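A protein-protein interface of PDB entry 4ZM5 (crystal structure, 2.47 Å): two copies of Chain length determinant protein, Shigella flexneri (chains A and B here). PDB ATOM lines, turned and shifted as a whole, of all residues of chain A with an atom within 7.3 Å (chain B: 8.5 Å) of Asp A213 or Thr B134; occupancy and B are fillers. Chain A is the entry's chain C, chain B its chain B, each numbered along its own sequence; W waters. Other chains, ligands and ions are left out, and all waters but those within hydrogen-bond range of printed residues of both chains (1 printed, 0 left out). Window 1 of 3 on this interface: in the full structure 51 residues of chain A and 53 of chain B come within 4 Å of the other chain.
Water W1 lies within hydrogen-bond range of OE1 of Glu B141 (2.6 Å), O of Tyr A205 (2.7 Å) and NE of Arg A208 (3.0 Å).
Printed residues of chain B that touch a printed residue of chain A: Arg B133, Thr B134, Val B137, Val B138 and Glu B141. Of the 17 printed residues of chain A, 5 touch a printed residue of chain B. Hydrophobic or aromatic side chains of chain A that line the printed part of chain B: Tyr A205. Among the printed residues, Asp or Glu carboxylates within 4 Å of a Lys or Arg side-chain nitrogen of the other chain: Arg A208 with Glu B141 (3.1 Å) and Asp A213 with Arg B133 (3.9 Å).
No position is printed for both chains. Of the 7 pairs that touch across the chains among the printed residues, none has its exchanged pair printed and touching as well.
NH2 of Arg B133 is in salt-bridge range of OD1 of Asp A213 (3.9 Å). OE2 of Glu B141 lies within salt-bridge range of NH2 of Arg A208 (3.1 Å).
The backbone carbonyl oxygen of Gln A206 sits at hydrogen-bond distance from the side-chain amide nitrogen of Asn A210, 3.1 Å away. The backbone carbonyl oxygen of Asp B130 sits at hydrogen-bond distance from the side-chain hydroxyl of Thr B134 (2.7 Å). NH1 of Arg B133 lies within salt-bridge range of OD1 of Asp B130, at 3.0 Å. NE2 of Gln A209 is in hydrogen-bond range of OD1 of Asp A213, 3.0 Å away.
Among the printed residues, merely in contact across the chains: Tyr A205 with Glu B141, Gln A206 with Val B138, Gln A209 with Thr B134, Gln A209 with Val B137 and Asp A213 with Thr B134.
Of the printed residues of chain B, Arg A208 touches Glu B141 (3.1 Å). Of the printed residues of chain B, Asp A213 touches Arg B133 (3.9 Å) and Thr B134 (3.7 Å). Of the printed residues of chain A, Thr B134 touches Gln A209 and Asp A213. Printed residues of chain A within 4 Å of Val B137: Gln A209 (3.4 Å). The nearest printed residue of chain A that does not touch Thr B134 is Asn A210 (4.2 Å). The nearest printed residue of chain A that does not touch Glu B141 is Gln A209 (5.3 Å).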
ATOM      1  N   ALA A  26     -27.810  29.113  32.741  1.00  0.00           N
ATOM      2  CA  ALA A  26     -28.545  30.311  32.362  1.00  0.00           C
ATOM      3  C   ALA A  26     -27.596  31.418  31.936  1.00  0.00           C
ATOM      4  O   ALA A  26     -27.808  32.034  30.897  1.00  0.00           O
ATOM      5  CB  ALA A  26     -29.420  30.774  33.518  1.00  0.00           C
ATOM      6  N   VAL A  29     -26.075  30.664  28.565  1.00  0.00           N
ATOM      7  CA  VAL A  29     -27.074  30.889  27.508  1.00  0.00           C
ATOM      8  C   VAL A  29     -27.172  32.411  27.181  1.00  0.00           C
ATOM      9  O   VAL A  29     -27.198  32.790  26.006  1.00  0.00           O
ATOM     10  CB  VAL A  29     -28.440  30.271  27.906  1.00  0.00           C
ATOM     11  CG1 VAL A  29     -29.569  30.735  26.992  1.00  0.00           C
ATOM     12  CG2 VAL A  29     -28.358  28.748  27.924  1.00  0.00           C
ATOM     13  N   ILE A  30     -27.173  33.266  28.218  1.00  0.00           N
ATOM     14  CA  ILE A  30     -27.240  34.725  28.037  1.00  0.00           C
ATOM     15  C   ILE A  30     -25.885  35.296  27.510  1.00  0.00           C
ATOM     16  O   ILE A  30     -25.905  36.073  26.553  1.00  0.00           O
ATOM     17  CB  ILE A  30     -27.670  35.463  29.351  1.00  0.00           C
ATOM     18  CG1 ILE A  30     -29.012  34.947  29.904  1.00  0.00           C
ATOM     19  CG2 ILE A  30     -27.687  36.991  29.156  1.00  0.00           C
ATOM     20  CD1 ILE A  30     -29.151  35.073  31.426  1.00  0.00           C
ATOM     21  N   TYR A 205     -29.116  33.920  11.910  1.00  0.00           N
ATOM     22  CA  TYR A 205     -29.715  32.668  12.361  1.00  0.00           C
ATOM     23  C   TYR A 205     -29.213  32.256  13.708  1.00  0.00           C
ATOM     24  O   TYR A 205     -29.998  31.740  14.503  1.00  0.00           O
ATOM     25  CB  TYR A 205     -29.461  31.551  11.352  1.00  0.00           C
ATOM     26  CG  TYR A 205     -30.142  31.792  10.030  1.00  0.00           C
ATOM     27  CD1 TYR A 205     -31.517  31.995   9.959  1.00  0.00           C
ATOM     28  CD2 TYR A 205     -29.417  31.805   8.841  1.00  0.00           C
ATOM     29  CE1 TYR A 205     -32.157  32.211   8.744  1.00  0.00           C
ATOM     30  CE2 TYR A 205     -30.047  32.019   7.614  1.00  0.00           C
ATOM     31  CZ  TYR A 205     -31.420  32.231   7.571  1.00  0.00           C
ATOM     32  OH  TYR A 205     -32.069  32.450   6.376  1.00  0.00           O
ATOM     33  N   GLN A 206     -27.919  32.488  13.982  1.00  0.00           N
ATOM     34  CA  GLN A 206     -27.303  32.213  15.270  1.00  0.00           C
ATOM     35  C   GLN A 206     -27.973  33.098  16.321  1.00  0.00           C
ATOM     36  O   GLN A 206     -28.501  32.566  17.304  1.00  0.00           O
ATOM     37  CB  GLN A 206     -25.795  32.456  15.173  1.00  0.00           C
ATOM     38  CG  GLN A 206     -25.010  32.193  16.449  1.00  0.00           C
ATOM     39  CD  GLN A 206     -23.944  33.251  16.654  1.00  0.00           C
ATOM     40  OE1 GLN A 206     -22.762  33.043  16.342  1.00  0.00           O
ATOM     41  NE2 GLN A 206     -24.345  34.416  17.174  1.00  0.00           N
ATOM     42  N   THR A 207     -28.055  34.430  16.053  1.00  0.00           N
ATOM     43  CA  THR A 207     -28.677  35.443  16.921  1.00  0.00           C
ATOM     44  C   THR A 207     -30.119  35.061  17.246  1.00  0.00           C
ATOM     45  O   THR A 207     -30.513  35.152  18.413  1.00  0.00           O
ATOM     46  CB  THR A 207     -28.594  36.838  16.271  1.00  0.00           C
ATOM     47  OG1 THR A 207     -27.246  37.099  15.899  1.00  0.00           O
ATOM     48  CG2 THR A 207     -29.087  37.964  17.188  1.00  0.00           C
ATOM     49  N   ARG A 208     -30.890  34.625  16.223  1.00  0.00           N
ATOM     50  CA  ARG A 208     -32.287  34.234  16.345  1.00  0.00           C
ATOM     51  C   ARG A 208     -32.451  32.983  17.227  1.00  0.00           C
ATOM     52  O   ARG A 208     -33.426  32.891  17.965  1.00  0.00           O
ATOM     53  CB  ARG A 208     -32.875  33.984  14.936  1.00  0.00           C
ATOM     54  CG  ARG A 208     -34.391  33.852  14.898  1.00  0.00           C
ATOM     55  CD  ARG A 208     -34.911  33.848  13.494  1.00  0.00           C
ATOM     56  NE  ARG A 208     -34.516  32.642  12.769  1.00  0.00           N
ATOM     57  CZ  ARG A 208     -34.950  32.326  11.554  1.00  0.00           C
ATOM     58  NH1 ARG A 208     -35.813  33.114  10.922  1.00  0.00           N
ATOM     59  NH2 ARG A 208     -34.545  31.211  10.969  1.00  0.00           N
ATOM     60  N   GLN A 209     -31.514  32.023  17.133  1.00  0.00           N
ATOM     61  CA  GLN A 209     -31.535  30.783  17.904  1.00  0.00           C
ATOM     62  C   GLN A 209     -31.181  31.071  19.358  1.00  0.00           C
ATOM     63  O   GLN A 209     -31.815  30.515  20.263  1.00  0.00           O
ATOM     64  CB  GLN A 209     -30.573  29.743  17.289  1.00  0.00           C
ATOM     65  CG  GLN A 209     -30.633  28.345  17.910  1.00  0.00           C
ATOM     66  CD  GLN A 209     -32.030  27.783  18.055  1.00  0.00           C
ATOM     67  OE1 GLN A 209     -32.841  27.786  17.119  1.00  0.00           O
ATOM     68  NE2 GLN A 209     -32.335  27.278  19.243  1.00  0.00           N
ATOM     69  N   ASN A 210     -30.171  31.963  19.564  1.00  0.00           N
ATOM     70  CA  ASN A 210     -29.698  32.408  20.872  1.00  0.00           C
ATOM     71  C   ASN A 210     -30.839  33.048  21.659  1.00  0.00           C
ATOM     72  O   ASN A 210     -30.955  32.828  22.870  1.00  0.00           O
ATOM     73  CB  ASN A 210     -28.535  33.405  20.711  1.00  0.00           C
ATOM     74  CG  ASN A 210     -27.250  32.805  20.190  1.00  0.00           C
ATOM     75  OD1 ASN A 210     -26.886  31.660  20.496  1.00  0.00           O
ATOM     76  ND2 ASN A 210     -26.520  33.588  19.406  1.00  0.00           N
ATOM     77  N   LEU A 211     -31.677  33.842  20.956  1.00  0.00           N
ATOM     78  CA  LEU A 211     -32.830  34.526  21.507  1.00  0.00           C
ATOM     79  C   LEU A 211     -33.882  33.515  21.931  1.00  0.00           C
ATOM     80  O   LEU A 211     -34.467  33.702  22.988  1.00  0.00           O
ATOM     81  CB  LEU A 211     -33.421  35.524  20.487  1.00  0.00           C
ATOM     82  CG  LEU A 211     -34.591  36.380  21.001  1.00  0.00           C
ATOM     83  CD1 LEU A 211     -34.216  37.170  22.270  1.00  0.00           C
ATOM     84  CD2 LEU A 211     -35.139  37.233  19.933  1.00  0.00           C
ATOM     85  N   LEU A 212     -34.108  32.449  21.128  1.00  0.00           N
ATOM     86  CA  LEU A 212     -35.048  31.374  21.417  1.00  0.00           C
ATOM     87  C   LEU A 212     -34.665  30.663  22.701  1.00  0.00           C
ATOM     88  O   LEU A 212     -35.549  30.349  23.495  1.00  0.00           O
ATOM     89  CB  LEU A 212     -35.087  30.354  20.258  1.00  0.00           C
ATOM     90  CG  LEU A 212     -36.146  30.533  19.195  1.00  0.00           C
ATOM     91  CD1 LEU A 212     -36.019  29.455  18.150  1.00  0.00           C
ATOM     92  CD2 LEU A 212     -37.559  30.456  19.789  1.00  0.00           C
ATOM     93  N   ASP A 213     -33.352  30.411  22.896  1.00  0.00           N
ATOM     94  CA  ASP A 213     -32.790  29.707  24.044  1.00  0.00           C
ATOM     95  C   ASP A 213     -32.900  30.537  25.335  1.00  0.00           C
ATOM     96  O   ASP A 213     -33.086  29.958  26.414  1.00  0.00           O
ATOM     97  CB  ASP A 213     -31.319  29.328  23.763  1.00  0.00           C
ATOM     98  CG  ASP A 213     -31.098  28.374  22.594  1.00  0.00           C
ATOM     99  OD1 ASP A 213     -32.053  27.630  22.235  1.00  0.00           O
ATOM    100  OD2 ASP A 213     -29.953  28.341  22.059  1.00  0.00           O
ATOM    101  N   ILE A 214     -32.799  31.879  25.219  1.00  0.00           N
ATOM    102  CA  ILE A 214     -32.920  32.804  26.350  1.00  0.00           C
ATOM    103  C   ILE A 214     -34.379  32.803  26.842  1.00  0.00           C
ATOM    104  O   ILE A 214     -34.616  32.809  28.048  1.00  0.00           O
ATOM    105  CB  ILE A 214     -32.382  34.232  26.018  1.00  0.00           C
ATOM    106  CG1 ILE A 214     -30.817  34.211  25.907  1.00  0.00           C
ATOM    107  CG2 ILE A 214     -32.833  35.247  27.088  1.00  0.00           C
ATOM    108  CD1 ILE A 214     -30.142  35.526  25.553  1.00  0.00           C
ATOM    109  N   GLU A 215     -35.338  32.730  25.915  1.00  0.00           N
ATOM    110  CA  GLU A 215     -36.764  32.678  26.215  1.00  0.00           C
ATOM    111  C   GLU A 215     -37.171  31.389  26.923  1.00  0.00           C
ATOM    112  O   GLU A 215     -38.227  31.369  27.554  1.00  0.00           O
ATOM    113  CB  GLU A 215     -37.566  32.808  24.935  1.00  0.00           C
ATOM    114  CG  GLU A 215     -38.157  34.184  24.724  1.00  0.00           C
ATOM    115  CD  GLU A 215     -38.227  34.599  23.270  1.00  0.00           C
ATOM    116  OE1 GLU A 215     -38.699  33.804  22.421  1.00  0.00           O
ATOM    117  OE2 GLU A 215     -37.765  35.723  22.976  1.00  0.00           O
ATOM    118  N   LYS A 216     -36.349  30.329  26.821  1.00  0.00           N
ATOM    119  CA  LYS A 216     -36.575  29.026  27.456  1.00  0.00           C
ATOM    120  C   LYS A 216     -36.146  29.022  28.928  1.00  0.00           C
ATOM    121  O   LYS A 216     -36.526  28.101  29.662  1.00  0.00           O
ATOM    122  CB  LYS A 216     -35.832  27.917  26.696  1.00  0.00           C
ATOM    123  CG  LYS A 216     -36.514  27.487  25.410  1.00  0.00           C
ATOM    124  CD  LYS A 216     -35.494  27.003  24.392  1.00  0.00           C
ATOM    125  CE  LYS A 216     -36.043  25.949  23.457  1.00  0.00           C
ATOM    126  NZ  LYS A 216     -36.991  26.493  22.435  1.00  0.00           N
ATOM    127  N   LEU A 217     -35.377  30.049  29.362  1.00  0.00           N
ATOM    128  CA  LEU A 217     -34.873  30.160  30.738  1.00  0.00           C
ATOM    129  C   LEU A 217     -35.957  30.570  31.731  1.00  0.00           C
ATOM    130  O   LEU A 217     -36.719  31.496  31.463  1.00  0.00           O
ATOM    131  CB  LEU A 217     -33.712  31.166  30.827  1.00  0.00           C
ATOM    132  CG  LEU A 217     -32.440  30.895  30.013  1.00  0.00           C
ATOM    133  CD1 LEU A 217     -31.524  32.115  30.020  1.00  0.00           C
ATOM    134  CD2 LEU A 217     -31.713  29.668  30.519  1.00  0.00           C
ATOM    135  N   LYS A 218     -35.989  29.928  32.905  1.00  0.00           N
ATOM    136  CA  LYS A 218     -36.956  30.267  33.956  1.00  0.00           C
ATOM    137  C   LYS A 218     -36.340  29.976  35.313  1.00  0.00           C
ATOM    138  O   LYS A 218     -35.946  28.837  35.562  1.00  0.00           O
ATOM    139  CB  LYS A 218     -38.324  29.550  33.770  1.00  0.00           C
ATOM    140  CG  LYS A 218     -38.286  28.204  33.035  1.00  0.00           C
ATOM    141  CD  LYS A 218     -39.649  27.779  32.492  1.00  0.00           C
ATOM    142  CE  LYS A 218     -39.822  28.102  31.023  1.00  0.00           C
ATOM    143  NZ  LYS A 218     -41.144  27.656  30.505  1.00  0.00           N
ATOM    144  N   LYS B 126     -24.227  19.428  28.911  1.00  0.00           N
ATOM    145  CA  LYS B 126     -25.294  20.372  28.621  1.00  0.00           C
ATOM    146  C   LYS B 126     -24.773  21.512  27.751  1.00  0.00           C
ATOM    147  O   LYS B 126     -25.394  21.809  26.734  1.00  0.00           O
ATOM    148  CB  LYS B 126     -25.892  20.923  29.941  1.00  0.00           C
ATOM    149  CG  LYS B 126     -26.940  22.053  29.796  1.00  0.00           C
ATOM    150  CD  LYS B 126     -28.320  21.560  29.392  1.00  0.00           C
ATOM    151  CE  LYS B 126     -29.362  22.649  29.505  1.00  0.00           C
ATOM    152  NZ  LYS B 126     -29.881  22.788  30.896  1.00  0.00           N
ATOM    153  N   ASN B 127     -23.625  22.122  28.123  1.00  0.00           N
ATOM    154  CA  ASN B 127     -23.053  23.255  27.379  1.00  0.00           C
ATOM    155  C   ASN B 127     -22.622  22.873  25.949  1.00  0.00           C
ATOM    156  O   ASN B 127     -22.897  23.633  25.008  1.00  0.00           O
ATOM    157  CB  ASN B 127     -21.873  23.874  28.147  1.00  0.00           C
ATOM    158  CG  ASN B 127     -22.242  24.531  29.471  1.00  0.00           C
ATOM    159  OD1 ASN B 127     -23.383  24.982  29.696  1.00  0.00           O
ATOM    160  ND2 ASN B 127     -21.261  24.641  30.363  1.00  0.00           N
ATOM    161  N   LEU B 128     -21.985  21.689  25.793  1.00  0.00           N
ATOM    162  CA  LEU B 128     -21.521  21.179  24.499  1.00  0.00           C
ATOM    163  C   LEU B 128     -22.678  20.734  23.594  1.00  0.00           C
ATOM    164  O   LEU B 128     -22.621  20.988  22.393  1.00  0.00           O
ATOM    165  CB  LEU B 128     -20.513  20.038  24.652  1.00  0.00           C
ATOM    166  CG  LEU B 128     -19.153  20.399  25.271  1.00  0.00           C
ATOM    167  CD1 LEU B 128     -18.234  19.232  25.199  1.00  0.00           C
ATOM    168  CD2 LEU B 128     -18.480  21.586  24.569  1.00  0.00           C
ATOM    169  N   GLN B 129     -23.724  20.107  24.167  1.00  0.00           N
ATOM    170  CA  GLN B 129     -24.908  19.666  23.426  1.00  0.00           C
ATOM    171  C   GLN B 129     -25.708  20.880  22.954  1.00  0.00           C
ATOM    172  O   GLN B 129     -26.226  20.852  21.835  1.00  0.00           O
ATOM    173  CB  GLN B 129     -25.781  18.733  24.271  1.00  0.00           C
ATOM    174  CG  GLN B 129     -25.186  17.335  24.403  1.00  0.00           C
ATOM    175  CD  GLN B 129     -25.873  16.446  25.417  1.00  0.00           C
ATOM    176  OE1 GLN B 129     -26.434  16.901  26.432  1.00  0.00           O
ATOM    177  NE2 GLN B 129     -25.774  15.143  25.191  1.00  0.00           N
ATOM    178  N   ASP B 130     -25.766  21.955  23.788  1.00  0.00           N
ATOM    179  CA  ASP B 130     -26.428  23.213  23.464  1.00  0.00           C
ATOM    180  C   ASP B 130     -25.711  23.889  22.296  1.00  0.00           C
ATOM    181  O   ASP B 130     -26.363  24.413  21.393  1.00  0.00           O
ATOM    182  CB  ASP B 130     -26.472  24.142  24.689  1.00  0.00           C
ATOM    183  CG  ASP B 130     -27.544  23.843  25.733  1.00  0.00           C
ATOM    184  OD1 ASP B 130     -28.056  22.696  25.757  1.00  0.00           O
ATOM    185  OD2 ASP B 130     -27.823  24.740  26.571  1.00  0.00           O
ATOM    186  N   SER B 131     -24.371  23.838  22.307  1.00  0.00           N
ATOM    187  CA  SER B 131     -23.498  24.397  21.278  1.00  0.00           C
ATOM    188  C   SER B 131     -23.682  23.640  19.943  1.00  0.00           C
ATOM    189  O   SER B 131     -23.863  24.290  18.917  1.00  0.00           O
ATOM    190  CB  SER B 131     -22.040  24.358  21.742  1.00  0.00           C
ATOM    191  OG  SER B 131     -21.129  24.884  20.790  1.00  0.00           O
ATOM    192  N   LEU B 132     -23.683  22.283  19.963  1.00  0.00           N
ATOM    193  CA  LEU B 132     -23.848  21.464  18.744  1.00  0.00           C
ATOM    194  C   LEU B 132     -25.209  21.671  18.108  1.00  0.00           C
ATOM    195  O   LEU B 132     -25.276  21.829  16.895  1.00  0.00           O
ATOM    196  CB  LEU B 132     -23.629  19.963  18.986  1.00  0.00           C
ATOM    197  CG  LEU B 132     -22.240  19.527  19.406  1.00  0.00           C
ATOM    198  CD1 LEU B 132     -22.271  18.124  19.944  1.00  0.00           C
ATOM    199  CD2 LEU B 132     -21.199  19.700  18.281  1.00  0.00           C
ATOM    200  N   ARG B 133     -26.277  21.681  18.928  1.00  0.00           N
ATOM    201  CA  ARG B 133     -27.675  21.889  18.538  1.00  0.00           C
ATOM    202  C   ARG B 133     -27.836  23.218  17.792  1.00  0.00           C
ATOM    203  O   ARG B 133     -28.368  23.227  16.675  1.00  0.00           O
ATOM    204  CB  ARG B 133     -28.566  21.845  19.780  1.00  0.00           C
ATOM    205  CG  ARG B 133     -30.052  21.935  19.504  1.00  0.00           C
ATOM    206  CD  ARG B 133     -30.832  21.742  20.796  1.00  0.00           C
ATOM    207  NE  ARG B 133     -30.910  22.964  21.601  1.00  0.00           N
ATOM    208  CZ  ARG B 133     -30.363  23.117  22.801  1.00  0.00           C
ATOM    209  NH1 ARG B 133     -29.722  22.107  23.382  1.00  0.00           N
ATOM    210  NH2 ARG B 133     -30.488  24.267  23.451  1.00  0.00           N
ATOM    211  N   THR B 134     -27.341  24.319  18.396  1.00  0.00           N
ATOM    212  CA  THR B 134     -27.376  25.675  17.840  1.00  0.00           C
ATOM    213  C   THR B 134     -26.701  25.709  16.478  1.00  0.00           C
ATOM    214  O   THR B 134     -27.252  26.245  15.527  1.00  0.00           O
ATOM    215  CB  THR B 134     -26.693  26.648  18.807  1.00  0.00           C
ATOM    216  OG1 THR B 134     -27.363  26.594  20.069  1.00  0.00           O
ATOM    217  CG2 THR B 134     -26.663  28.087  18.284  1.00  0.00           C
ATOM    218  N   GLN B 135     -25.503  25.127  16.400  1.00  0.00           N
ATOM    219  CA  GLN B 135     -24.677  25.063  15.203  1.00  0.00           C
ATOM    220  C   GLN B 135     -25.369  24.258  14.105  1.00  0.00           C
ATOM    221  O   GLN B 135     -25.321  24.670  12.954  1.00  0.00           O
ATOM    222  CB  GLN B 135     -23.302  24.486  15.545  1.00  0.00           C
ATOM    223  CG  GLN B 135     -22.440  25.470  16.336  1.00  0.00           C
ATOM    224  CD  GLN B 135     -21.049  24.935  16.605  1.00  0.00           C
ATOM    225  OE1 GLN B 135     -20.752  24.410  17.689  1.00  0.00           O
ATOM    226  NE2 GLN B 135     -20.150  25.100  15.638  1.00  0.00           N
ATOM    227  N   GLU B 136     -26.073  23.176  14.470  1.00  0.00           N
ATOM    228  CA  GLU B 136     -26.832  22.319  13.558  1.00  0.00           C
ATOM    229  C   GLU B 136     -28.033  23.067  13.003  1.00  0.00           C
ATOM    230  O   GLU B 136     -28.280  22.977  11.806  1.00  0.00           O
ATOM    231  CB  GLU B 136     -27.292  21.037  14.265  1.00  0.00           C
ATOM    232  CG  GLU B 136     -26.207  19.983  14.364  1.00  0.00           C
ATOM    233  CD  GLU B 136     -26.290  19.031  15.544  1.00  0.00           C
ATOM    234  OE1 GLU B 136     -27.243  19.132  16.351  1.00  0.00           O
ATOM    235  OE2 GLU B 136     -25.387  18.172  15.655  1.00  0.00           O
ATOM    236  N   VAL B 137     -28.755  23.843  13.858  1.00  0.00           N
ATOM    237  CA  VAL B 137     -29.921  24.647  13.450  1.00  0.00           C
ATOM    238  C   VAL B 137     -29.462  25.667  12.387  1.00  0.00           C
ATOM    239  O   VAL B 137     -30.067  25.730  11.302  1.00  0.00           O
ATOM    240  CB  VAL B 137     -30.640  25.319  14.667  1.00  0.00           C
ATOM    241  CG1 VAL B 137     -31.650  26.374  14.230  1.00  0.00           C
ATOM    242  CG2 VAL B 137     -31.312  24.278  15.566  1.00  0.00           C
ATOM    243  N   VAL B 138     -28.361  26.407  12.682  1.00  0.00           N
ATOM    244  CA  VAL B 138     -27.772  27.418  11.788  1.00  0.00           C
ATOM    245  C   VAL B 138     -27.410  26.794  10.434  1.00  0.00           C
ATOM    246  O   VAL B 138     -27.832  27.314   9.398  1.00  0.00           O
ATOM    247  CB  VAL B 138     -26.540  28.135  12.420  1.00  0.00           C
ATOM    248  CG1 VAL B 138     -25.905  29.113  11.430  1.00  0.00           C
ATOM    249  CG2 VAL B 138     -26.922  28.858  13.711  1.00  0.00           C
ATOM    250  N   ALA B 139     -26.660  25.672  10.443  1.00  0.00           N
ATOM    251  CA  ALA B 139     -26.211  24.985   9.221  1.00  0.00           C
ATOM    252  C   ALA B 139     -27.383  24.511   8.360  1.00  0.00           C
ATOM    253  O   ALA B 139     -27.279  24.531   7.131  1.00  0.00           O
ATOM    254  CB  ALA B 139     -25.312  23.818   9.564  1.00  0.00           C
ATOM    255  N   GLN B 140     -28.501  24.123   9.003  1.00  0.00           N
ATOM    256  CA  GLN B 140     -29.707  23.665   8.330  1.00  0.00           C
ATOM    257  C   GLN B 140     -30.438  24.860   7.705  1.00  0.00           C
ATOM    258  O   GLN B 140     -30.867  24.752   6.553  1.00  0.00           O
ATOM    259  CB  GLN B 140     -30.615  22.870   9.286  1.00  0.00           C
ATOM    260  CG  GLN B 140     -31.866  22.256   8.650  1.00  0.00           C
ATOM    261  CD  GLN B 140     -31.553  21.260   7.576  1.00  0.00           C
ATOM    262  OE1 GLN B 140     -31.867  21.484   6.409  1.00  0.00           O
ATOM    263  NE2 GLN B 140     -30.926  20.144   7.933  1.00  0.00           N
ATOM    264  N   GLU B 141     -30.540  25.995   8.442  1.00  0.00           N
ATOM    265  CA  GLU B 141     -31.191  27.218   7.979  1.00  0.00           C
ATOM    266  C   GLU B 141     -30.427  27.821   6.783  1.00  0.00           C
ATOM    267  O   GLU B 141     -31.043  28.295   5.824  1.00  0.00           O
ATOM    268  CB  GLU B 141     -31.348  28.215   9.137  1.00  0.00           C
ATOM    269  CG  GLU B 141     -32.488  27.812  10.064  1.00  0.00           C
ATOM    270  CD  GLU B 141     -32.627  28.499  11.405  1.00  0.00           C
ATOM    271  OE1 GLU B 141     -31.617  29.038  11.911  1.00  0.00           O
ATOM    272  OE2 GLU B 141     -33.738  28.441  11.980  1.00  0.00           O
ATOM    273  N   PHE B 200     -20.539  23.126   8.540  1.00  0.00           N
ATOM    274  CA  PHE B 200     -20.342  23.581   9.920  1.00  0.00           C
ATOM    275  C   PHE B 200     -18.992  24.244  10.086  1.00  0.00           C
ATOM    276  O   PHE B 200     -18.047  23.888   9.371  1.00  0.00           O
ATOM    277  CB  PHE B 200     -20.407  22.398  10.890  1.00  0.00           C
ATOM    278  CG  PHE B 200     -21.620  21.526  10.832  1.00  0.00           C
ATOM    279  CD1 PHE B 200     -22.799  21.902  11.468  1.00  0.00           C
ATOM    280  CD2 PHE B 200     -21.577  20.305  10.174  1.00  0.00           C
ATOM    281  CE1 PHE B 200     -23.918  21.072  11.433  1.00  0.00           C
ATOM    282  CE2 PHE B 200     -22.695  19.483  10.130  1.00  0.00           C
ATOM    283  CZ  PHE B 200     -23.853  19.865  10.768  1.00  0.00           C
ATOM    284  N   TYR B 204     -17.390  23.244  15.330  1.00  0.00           N
ATOM    285  CA  TYR B 204     -18.380  22.169  15.401  1.00  0.00           C
ATOM    286  C   TYR B 204     -17.731  20.802  15.661  1.00  0.00           C
ATOM    287  O   TYR B 204     -18.151  20.088  16.583  1.00  0.00           O
ATOM    288  CB  TYR B 204     -19.239  22.116  14.128  1.00  0.00           C
ATOM    289  CG  TYR B 204     -20.285  21.024  14.173  1.00  0.00           C
ATOM    290  CD1 TYR B 204     -21.454  21.176  14.927  1.00  0.00           C
ATOM    291  CD2 TYR B 204     -20.101  19.828  13.482  1.00  0.00           C
ATOM    292  CE1 TYR B 204     -22.407  20.160  14.996  1.00  0.00           C
ATOM    293  CE2 TYR B 204     -21.063  18.814  13.524  1.00  0.00           C
ATOM    294  CZ  TYR B 204     -22.203  18.980  14.301  1.00  0.00           C
ATOM    295  OH  TYR B 204     -23.147  17.993  14.341  1.00  0.00           O
HETATM  296  O   HOH W   1     -32.409  30.697  13.763  1.00  0.00           O
